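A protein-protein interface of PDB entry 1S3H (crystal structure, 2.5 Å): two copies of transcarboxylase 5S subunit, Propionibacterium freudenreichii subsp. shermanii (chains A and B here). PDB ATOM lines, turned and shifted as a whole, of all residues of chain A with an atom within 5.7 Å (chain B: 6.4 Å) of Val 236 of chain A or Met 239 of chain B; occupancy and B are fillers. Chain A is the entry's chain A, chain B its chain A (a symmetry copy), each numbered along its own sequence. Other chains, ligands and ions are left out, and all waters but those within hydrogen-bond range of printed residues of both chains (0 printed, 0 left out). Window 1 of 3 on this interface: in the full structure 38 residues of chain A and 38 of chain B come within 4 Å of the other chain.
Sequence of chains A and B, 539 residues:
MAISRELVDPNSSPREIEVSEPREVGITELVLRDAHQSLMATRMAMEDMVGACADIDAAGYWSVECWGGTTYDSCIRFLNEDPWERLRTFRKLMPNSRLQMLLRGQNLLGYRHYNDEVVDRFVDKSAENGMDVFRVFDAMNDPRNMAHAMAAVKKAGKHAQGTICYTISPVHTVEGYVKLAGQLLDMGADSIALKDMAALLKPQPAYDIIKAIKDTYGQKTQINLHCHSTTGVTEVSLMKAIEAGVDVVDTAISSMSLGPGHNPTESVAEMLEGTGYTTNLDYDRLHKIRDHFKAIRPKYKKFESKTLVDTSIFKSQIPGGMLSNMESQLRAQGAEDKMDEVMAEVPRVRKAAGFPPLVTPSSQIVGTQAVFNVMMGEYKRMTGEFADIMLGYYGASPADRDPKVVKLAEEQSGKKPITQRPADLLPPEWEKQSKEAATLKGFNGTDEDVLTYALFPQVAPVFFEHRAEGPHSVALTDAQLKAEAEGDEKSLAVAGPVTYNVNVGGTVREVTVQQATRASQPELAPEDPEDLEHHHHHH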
ATOM      1  N   PRO A 203     -24.108   1.140  28.408  1.00  0.00           N
ATOM      2  CA  PRO A 203     -24.453   1.255  26.984  1.00  0.00           C
ATOM      3  C   PRO A 203     -25.911   1.489  26.583  1.00  0.00           C
ATOM      4  O   PRO A 203     -26.195   2.380  25.785  1.00  0.00           O
ATOM      5  CB  PRO A 203     -23.909  -0.039  26.393  1.00  0.00           C
ATOM      6  CG  PRO A 203     -22.718  -0.302  27.229  1.00  0.00           C
ATOM      7  CD  PRO A 203     -23.227  -0.021  28.628  1.00  0.00           C
ATOM      8  N   GLY A 232     -14.990   0.538  33.651  1.00  0.00           N
ATOM      9  CA  GLY A 232     -14.590  -0.216  32.475  1.00  0.00           C
ATOM     10  C   GLY A 232     -15.622  -0.526  31.420  1.00  0.00           C
ATOM     11  O   GLY A 232     -15.308  -1.276  30.497  1.00  0.00           O
ATOM     12  N   VAL A 233     -16.818   0.065  31.510  1.00  0.00           N
ATOM     13  CA  VAL A 233     -17.884  -0.213  30.534  1.00  0.00           C
ATOM     14  C   VAL A 233     -18.254   1.029  29.721  1.00  0.00           C
ATOM     15  O   VAL A 233     -19.112   0.959  28.842  1.00  0.00           O
ATOM     16  CB  VAL A 233     -19.209  -0.670  31.232  1.00  0.00           C
ATOM     17  CG1 VAL A 233     -18.924  -1.657  32.327  1.00  0.00           C
ATOM     18  CG2 VAL A 233     -19.953   0.537  31.795  1.00  0.00           C
ATOM     19  N   THR A 234     -17.609   2.159  29.970  1.00  0.00           N
ATOM     20  CA  THR A 234     -18.027   3.406  29.314  1.00  0.00           C
ATOM     21  C   THR A 234     -17.560   3.537  27.862  1.00  0.00           C
ATOM     22  O   THR A 234     -18.193   4.242  27.077  1.00  0.00           O
ATOM     23  CB  THR A 234     -17.576   4.597  30.126  1.00  0.00           C
ATOM     24  OG1 THR A 234     -16.152   4.567  30.263  1.00  0.00           O
ATOM     25  CG2 THR A 234     -18.214   4.535  31.504  1.00  0.00           C
ATOM     26  N   GLU A 235     -16.472   2.898  27.467  1.00  0.00           N
ATOM     27  CA  GLU A 235     -16.116   3.063  26.052  1.00  0.00           C
ATOM     28  C   GLU A 235     -17.194   2.421  25.174  1.00  0.00           C
ATOM     29  O   GLU A 235     -17.367   2.790  24.013  1.00  0.00           O
ATOM     30  CB  GLU A 235     -14.768   2.446  25.742  1.00  0.00           C
ATOM     31  CG  GLU A 235     -14.399   2.687  24.306  1.00  0.00           C
ATOM     32  CD  GLU A 235     -12.934   2.521  24.048  1.00  0.00           C
ATOM     33  OE1 GLU A 235     -12.138   3.135  24.769  1.00  0.00           O
ATOM     34  OE2 GLU A 235     -12.571   1.788  23.115  1.00  0.00           O
ATOM     35  N   VAL A 236     -17.922   1.445  25.708  1.00  0.00           N
ATOM     36  CA  VAL A 236     -18.974   0.803  24.907  1.00  0.00           C
ATOM     37  C   VAL A 236     -20.173   1.751  24.881  1.00  0.00           C
ATOM     38  O   VAL A 236     -20.932   1.811  23.916  1.00  0.00           O
ATOM     39  CB  VAL A 236     -19.391  -0.579  25.492  1.00  0.00           C
ATOM     40  CG1 VAL A 236     -20.353  -1.281  24.549  1.00  0.00           C
ATOM     41  CG2 VAL A 236     -18.171  -1.440  25.686  1.00  0.00           C
ATOM     42  N   SER A 237     -20.301   2.511  25.950  1.00  0.00           N
ATOM     43  CA  SER A 237     -21.385   3.495  26.071  1.00  0.00           C
ATOM     44  C   SER A 237     -21.144   4.609  25.050  1.00  0.00           C
ATOM     45  O   SER A 237     -22.076   5.143  24.453  1.00  0.00           O
ATOM     46  CB  SER A 237     -21.389   4.073  27.484  1.00  0.00           C
ATOM     47  OG  SER A 237     -21.450   3.021  28.424  1.00  0.00           O
ATOM     48  N   LEU A 238     -19.871   4.949  24.877  1.00  0.00           N
ATOM     49  CA  LEU A 238     -19.470   5.985  23.917  1.00  0.00           C
ATOM     50  C   LEU A 238     -19.911   5.549  22.519  1.00  0.00           C
ATOM     51  O   LEU A 238     -20.468   6.343  21.763  1.00  0.00           O
ATOM     52  CB  LEU A 238     -17.961   6.180  23.970  1.00  0.00           C
ATOM     53  CG  LEU A 238     -17.479   7.476  24.610  1.00  0.00           C
ATOM     54  CD1 LEU A 238     -18.181   7.696  25.934  1.00  0.00           C
ATOM     55  CD2 LEU A 238     -15.964   7.422  24.775  1.00  0.00           C
ATOM     56  N   MET A 239     -19.686   4.282  22.181  1.00  0.00           N
ATOM     57  CA  MET A 239     -20.103   3.794  20.858  1.00  0.00           C
ATOM     58  C   MET A 239     -21.626   3.887  20.761  1.00  0.00           C
ATOM     59  O   MET A 239     -22.175   4.329  19.754  1.00  0.00           O
ATOM     60  CB  MET A 239     -19.701   2.342  20.657  1.00  0.00           C
ATOM     61  CG  MET A 239     -20.053   1.818  19.273  1.00  0.00           C
ATOM     62  SD  MET A 239     -18.932   2.455  18.016  1.00  0.00           S
ATOM     63  CE  MET A 239     -19.953   3.579  17.142  1.00  0.00           C
ATOM     64  N   LYS A 240     -22.310   3.470  21.818  1.00  0.00           N
ATOM     65  CA  LYS A 240     -23.777   3.530  21.807  1.00  0.00           C
ATOM     66  C   LYS A 240     -24.268   4.978  21.756  1.00  0.00           C
ATOM     67  O   LYS A 240     -25.266   5.264  21.098  1.00  0.00           O
ATOM     68  CB  LYS A 240     -24.364   2.805  23.016  1.00  0.00           C
ATOM     69  CG  LYS A 240     -24.262   1.300  22.872  1.00  0.00           C
ATOM     70  CD  LYS A 240     -25.053   0.870  21.638  1.00  0.00           C
ATOM     71  CE  LYS A 240     -24.952  -0.608  21.374  1.00  0.00           C
ATOM     72  NZ  LYS A 240     -25.681  -0.912  20.125  1.00  0.00           N
ATOM     73  N   ALA A 241     -23.579   5.889  22.438  1.00  0.00           N
ATOM     74  CA  ALA A 241     -24.002   7.297  22.408  1.00  0.00           C
ATOM     75  C   ALA A 241     -23.854   7.828  20.981  1.00  0.00           C
ATOM     76  O   ALA A 241     -24.708   8.558  20.481  1.00  0.00           O
ATOM     77  CB  ALA A 241     -23.170   8.137  23.370  1.00  0.00           C
ATOM     78  N   THR B 234     -11.007  -3.165  21.712  1.00  0.00           N
ATOM     79  CA  THR B 234     -11.627  -4.492  21.589  1.00  0.00           C
ATOM     80  C   THR B 234     -12.874  -4.683  22.457  1.00  0.00           C
ATOM     81  O   THR B 234     -13.730  -5.503  22.126  1.00  0.00           O
ATOM     82  CB  THR B 234     -10.609  -5.570  21.879  1.00  0.00           C
ATOM     83  OG1 THR B 234     -10.089  -5.390  23.200  1.00  0.00           O
ATOM     84  CG2 THR B 234      -9.473  -5.470  20.874  1.00  0.00           C
ATOM     85  N   GLU B 235     -13.015  -3.971  23.562  1.00  0.00           N
ATOM     86  CA  GLU B 235     -14.254  -4.204  24.315  1.00  0.00           C
ATOM     87  C   GLU B 235     -15.454  -3.737  23.486  1.00  0.00           C
ATOM     88  O   GLU B 235     -16.575  -4.206  23.675  1.00  0.00           O
ATOM     89  CB  GLU B 235     -14.240  -3.482  25.647  1.00  0.00           C
ATOM     90  CG  GLU B 235     -15.487  -3.791  26.424  1.00  0.00           C
ATOM     91  CD  GLU B 235     -15.347  -3.501  27.885  1.00  0.00           C
ATOM     92  OE1 GLU B 235     -14.378  -3.979  28.488  1.00  0.00           O
ATOM     93  OE2 GLU B 235     -16.211  -2.807  28.442  1.00  0.00           O
ATOM     94  N   VAL B 236     -15.240  -2.801  22.566  1.00  0.00           N
ATOM     95  CA  VAL B 236     -16.358  -2.327  21.739  1.00  0.00           C
ATOM     96  C   VAL B 236     -16.620  -3.387  20.670  1.00  0.00           C
ATOM     97  O   VAL B 236     -17.746  -3.592  20.222  1.00  0.00           O
ATOM     98  CB  VAL B 236     -16.049  -0.953  21.073  1.00  0.00           C
ATOM     99  CG1 VAL B 236     -17.285  -0.420  20.369  1.00  0.00           C
ATOM    100  CG2 VAL B 236     -15.612   0.036  22.122  1.00  0.00           C
ATOM    101  N   SER B 237     -15.558  -4.075  20.301  1.00  0.00           N
ATOM    102  CA  SER B 237     -15.645  -5.149  19.303  1.00  0.00           C
ATOM    103  C   SER B 237     -16.445  -6.306  19.905  1.00  0.00           C
ATOM    104  O   SER B 237     -17.220  -6.972  19.221  1.00  0.00           O
ATOM    105  CB  SER B 237     -14.238  -5.620  18.941  1.00  0.00           C
ATOM    106  OG  SER B 237     -13.459  -4.512  18.540  1.00  0.00           O
ATOM    107  N   LEU B 238     -16.226  -6.532  21.196  1.00  0.00           N
ATOM    108  CA  LEU B 238     -16.932  -7.591  21.927  1.00  0.00           C
ATOM    109  C   LEU B 238     -18.434  -7.304  21.869  1.00  0.00           C
ATOM    110  O   LEU B 238     -19.232  -8.203  21.608  1.00  0.00           O
ATOM    111  CB  LEU B 238     -16.447  -7.632  23.370  1.00  0.00           C
ATOM    112  CG  LEU B 238     -15.575  -8.824  23.744  1.00  0.00           C
ATOM    113  CD1 LEU B 238     -14.481  -9.013  22.715  1.00  0.00           C
ATOM    114  CD2 LEU B 238     -15.005  -8.609  25.143  1.00  0.00           C
ATOM    115  N   MET B 239     -18.820  -6.050  22.086  1.00  0.00           N
ATOM    116  CA  MET B 239     -20.247  -5.704  22.026  1.00  0.00           C
ATOM    117  C   MET B 239     -20.751  -5.953  20.604  1.00  0.00           C
ATOM    118  O   MET B 239     -21.822  -6.520  20.397  1.00  0.00           O
ATOM    119  CB  MET B 239     -20.472  -4.238  22.360  1.00  0.00           C
ATOM    120  CG  MET B 239     -21.944  -3.855  22.377  1.00  0.00           C
ATOM    121  SD  MET B 239     -22.774  -4.469  23.851  1.00  0.00           S
ATOM    122  CE  MET B 239     -23.780  -5.750  23.205  1.00  0.00           C
ATOM    123  N   LYS B 240     -19.968  -5.529  19.620  1.00  0.00           N
ATOM    124  CA  LYS B 240     -20.377  -5.733  18.224  1.00  0.00           C
ATOM    125  C   LYS B 240     -20.419  -7.222  17.877  1.00  0.00           C
ATOM    126  O   LYS B 240     -21.296  -7.653  17.129  1.00  0.00           O
ATOM    127  CB  LYS B 240     -19.455  -4.983  17.268  1.00  0.00           C
ATOM    128  CG  LYS B 240     -19.712  -3.489  17.295  1.00  0.00           C
ATOM    129  CD  LYS B 240     -21.152  -3.231  16.856  1.00  0.00           C
ATOM    130  CE  LYS B 240     -21.522  -1.774  16.919  1.00  0.00           C
ATOM    131  NZ  LYS B 240     -22.947  -1.636  16.553  1.00  0.00           N
ATOM    132  N   ALA B 241     -19.488  -8.008  18.409  1.00  0.00           N
ATOM    133  CA  ALA B 241     -19.495  -9.450  18.117  1.00  0.00           C
ATOM    134  C   ALA B 241     -20.767 -10.067  18.701  1.00  0.00           C
ATOM    135  O   ALA B 241     -21.408 -10.912  18.080  1.00  0.00           O
ATOM    136  CB  ALA B 241     -18.264 -10.130  18.703  1.00  0.00           C
ATOM    137  N   ILE B 242     -21.139  -9.631  19.891  1.00  0.00           N
ATOM    138  CA  ILE B 242     -22.354 -10.152  20.531  1.00  0.00           C
ATOM    139  C   ILE B 242     -23.583  -9.741  19.716  1.00  0.00           C
ATOM    140  O   ILE B 242     -24.498 -10.539  19.527  1.00  0.00           O
ATOM    141  CB  ILE B 242     -22.444  -9.661  21.994  1.00  0.00           C
ATOM    142  CG1 ILE B 242     -21.406 -10.420  22.820  1.00  0.00           C
ATOM    143  CG2 ILE B 242     -23.854  -9.848  22.553  1.00  0.00           C
ATOM    144  CD1 ILE B 242     -21.182  -9.887  24.207  1.00  0.00           C
ATOM    145  N   GLU B 243     -23.623  -8.520  19.202  1.00  0.00           N
ATOM    146  CA  GLU B 243     -24.786  -8.118  18.398  1.00  0.00           C
ATOM    147  C   GLU B 243     -24.815  -8.958  17.120  1.00  0.00           C
ATOM    148  O   GLU B 243     -25.887  -9.274  16.605  1.00  0.00           O
ATOM    149  CB  GLU B 243     -24.713  -6.635  18.038  1.00  0.00           C
ATOM    150  CG  GLU B 243     -24.686  -5.730  19.259  1.00  0.00           C
ATOM    151  CD  GLU B 243     -24.493  -4.275  18.914  1.00  0.00           C
ATOM    152  OE1 GLU B 243     -23.694  -3.958  18.006  1.00  0.00           O
ATOM    153  OE2 GLU B 243     -25.134  -3.437  19.571  1.00  0.00           O
ATOM    154  N   ALA B 244     -23.629  -9.332  16.633  1.00  0.00           N
ATOM    155  CA  ALA B 244     -23.508 -10.135  15.407  1.00  0.00           C
ATOM    156  C   ALA B 244     -23.825 -11.601  15.709  1.00  0.00           C
ATOM    157  O   ALA B 244     -23.947 -12.425  14.804  1.00  0.00           O
ATOM    158  CB  ALA B 244     -22.100 -10.000  14.829  1.00  0.00           C
ATOM    159  N   MET B 271     -21.792  -4.335  31.304  1.00  0.00           N
ATOM    160  CA  MET B 271     -22.168  -3.453  30.189  1.00  0.00           C
ATOM    161  C   MET B 271     -23.409  -3.944  29.442  1.00  0.00           C
ATOM    162  O   MET B 271     -23.999  -3.175  28.686  1.00  0.00           O
ATOM    163  CB  MET B 271     -21.030  -3.343  29.167  1.00  0.00           C
ATOM    164  CG  MET B 271     -20.763  -4.644  28.435  1.00  0.00           C
ATOM    165  SD  MET B 271     -19.338  -4.609  27.361  1.00  0.00           S
ATOM    166  CE  MET B 271     -19.925  -5.561  26.027  1.00  0.00           C
ATOM    167  N   LEU B 272     -23.816  -5.193  29.636  1.00  0.00           N
ATOM    168  CA  LEU B 272     -24.951  -5.740  28.878  1.00  0.00           C
ATOM    169  C   LEU B 272     -26.308  -5.426  29.512  1.00  0.00           C
ATOM    170  O   LEU B 272     -27.334  -5.530  28.841  1.00  0.00           O
ATOM    171  CB  LEU B 272     -24.817  -7.260  28.740  1.00  0.00           C
ATOM    172  CG  LEU B 272     -23.617  -7.804  27.977  1.00  0.00           C
ATOM    173  CD1 LEU B 272     -23.665  -9.319  27.979  1.00  0.00           C
ATOM    174  CD2 LEU B 272     -23.647  -7.289  26.557  1.00  0.00           C
ATOM    175  N   THR B 275     -29.549  -4.665  27.468  1.00  0.00           N
ATOM    176  CA  THR B 275     -29.371  -4.836  26.018  1.00  0.00           C
ATOM    177  C   THR B 275     -30.217  -5.999  25.495  1.00  0.00           C
ATOM    178  O   THR B 275     -30.432  -6.129  24.291  1.00  0.00           O
ATOM    179  CB  THR B 275     -27.887  -5.146  25.660  1.00  0.00           C
ATOM    180  OG1 THR B 275     -27.473  -6.359  26.311  1.00  0.00           O
ATOM    181  CG2 THR B 275     -26.975  -4.009  26.103  1.00  0.00           C
ATOM    182  N   TYR B 277     -29.188  -8.826  26.092  1.00  0.00           N
ATOM    183  CA  TYR B 277     -28.135  -9.848  26.163  1.00  0.00           C
ATOM    184  C   TYR B 277     -27.779 -10.017  27.640  1.00  0.00           C
ATOM    185  O   TYR B 277     -27.845  -9.059  28.407  1.00  0.00           O
ATOM    186  CB  TYR B 277     -26.906  -9.402  25.390  1.00  0.00           C
ATOM    187  CG  TYR B 277     -27.201  -9.152  23.951  1.00  0.00           C
ATOM    188  CD1 TYR B 277     -26.946  -7.911  23.381  1.00  0.00           C
ATOM    189  CD2 TYR B 277     -27.734 -10.160  23.151  1.00  0.00           C
ATOM    190  CE1 TYR B 277     -27.203  -7.671  22.048  1.00  0.00           C
ATOM    191  CE2 TYR B 277     -28.000  -9.937  21.811  1.00  0.00           C
ATOM    192  CZ  TYR B 277     -27.724  -8.687  21.261  1.00  0.00           C
ATOM    193  OH  TYR B 277     -27.918  -8.473  19.922  1.00  0.00           O
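O of Val 233 of chain A sits at hydrogen-bond distance from OG of Ser 237 of chain A (3.1 Å). The side-chain amino group (NZ) of Lys 240 of chain B is in salt-bridge range of the side-chain carboxylate (OE1) of Glu 243 of chain B (2.8 Å).
Among the printed residues, pairs that only touch across the chains: Pro 203 of chain A with Met 271 of chain B, Glu 235 of chain A with Val 236 of chain B, Val 236 of chain A with Glu 235 of chain B, Met 239 of chain A with Val 236 of chain B, Val 236 of chain A with Met 239 of chain B, Val 233 of chain A with Glu 235 of chain B, Val 236 of chain A with Met 271 of chain B and Val 233 of chain A with Met 271 of chain B.
Hydrophobic or aromatic side chains of chain A within 4 Å of the printed part of chain B: Pro 203, Val 233, Val 236 and Met 239. Of the 15 printed residues of chain B, 5 touch a printed residue of chain A. Among the printed residues, 10 pairs touch across the chains. Among the printed residues, Asp or Glu carboxylates within 4 Å of a Lys or Arg side-chain nitrogen of the other chain: Lys 240 of chain A with Glu 243 of chain B (2.6 Å).
Glu 235 of chain A touches Val 236 of chain B, and with the chains exchanged Val 236 of chain A touches Glu 235 of chain B. Val 236 of chain A touches Met 239 of chain B, and with the chains exchanged Met 239 of chain A touches Val 236 of chain B. Of the 10 pairs that touch across the chains among the printed residues, 4 have their exchanged pair printed and touching as well.
Of the printed residues of chain B, Gly 232 of chain A touches Glu 235. Of the printed residues of chain B, Val 233 of chain A touches Glu 235 (3.7 Å) and Met 271 (3.8 Å). Val 236 of chain A touches just these residues of chain B: Glu 235 (3.6 Å), Met 239 (3.7 Å) and Met 271 (3.8 Å). Printed residues of chain B within 4 Å of Met 239 of chain A: Val 236. Of the printed residues of chain B, Lys 240 of chain A touches Glu 243. Of chain A, only Val 236 comes within 4 Å of Met 239 of chain B. Ala 241 of chain B touches none of the printed residues of chain A. Ala 244 of chain B touches none of the printed residues of chain A. Of the printed residues of chain A, Met 271 of chain B touches Pro 203, Val 233 and Val 236. The nearest residue of chain A that does not touch Met 239 of chain B is Lys 240 of chain A (4.5 Å).
The side-chain carboxylate of Glu 235 of chain B sits close to the backbone carbonyl oxygen of Gly 232 of chain A (2.7 Å). The side-chain amino group (NZ) of Lys 240 of chain A lies within salt-bridge range of the side-chain carboxylate (OE2) of Glu 243 of chain B (2.6 Å).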
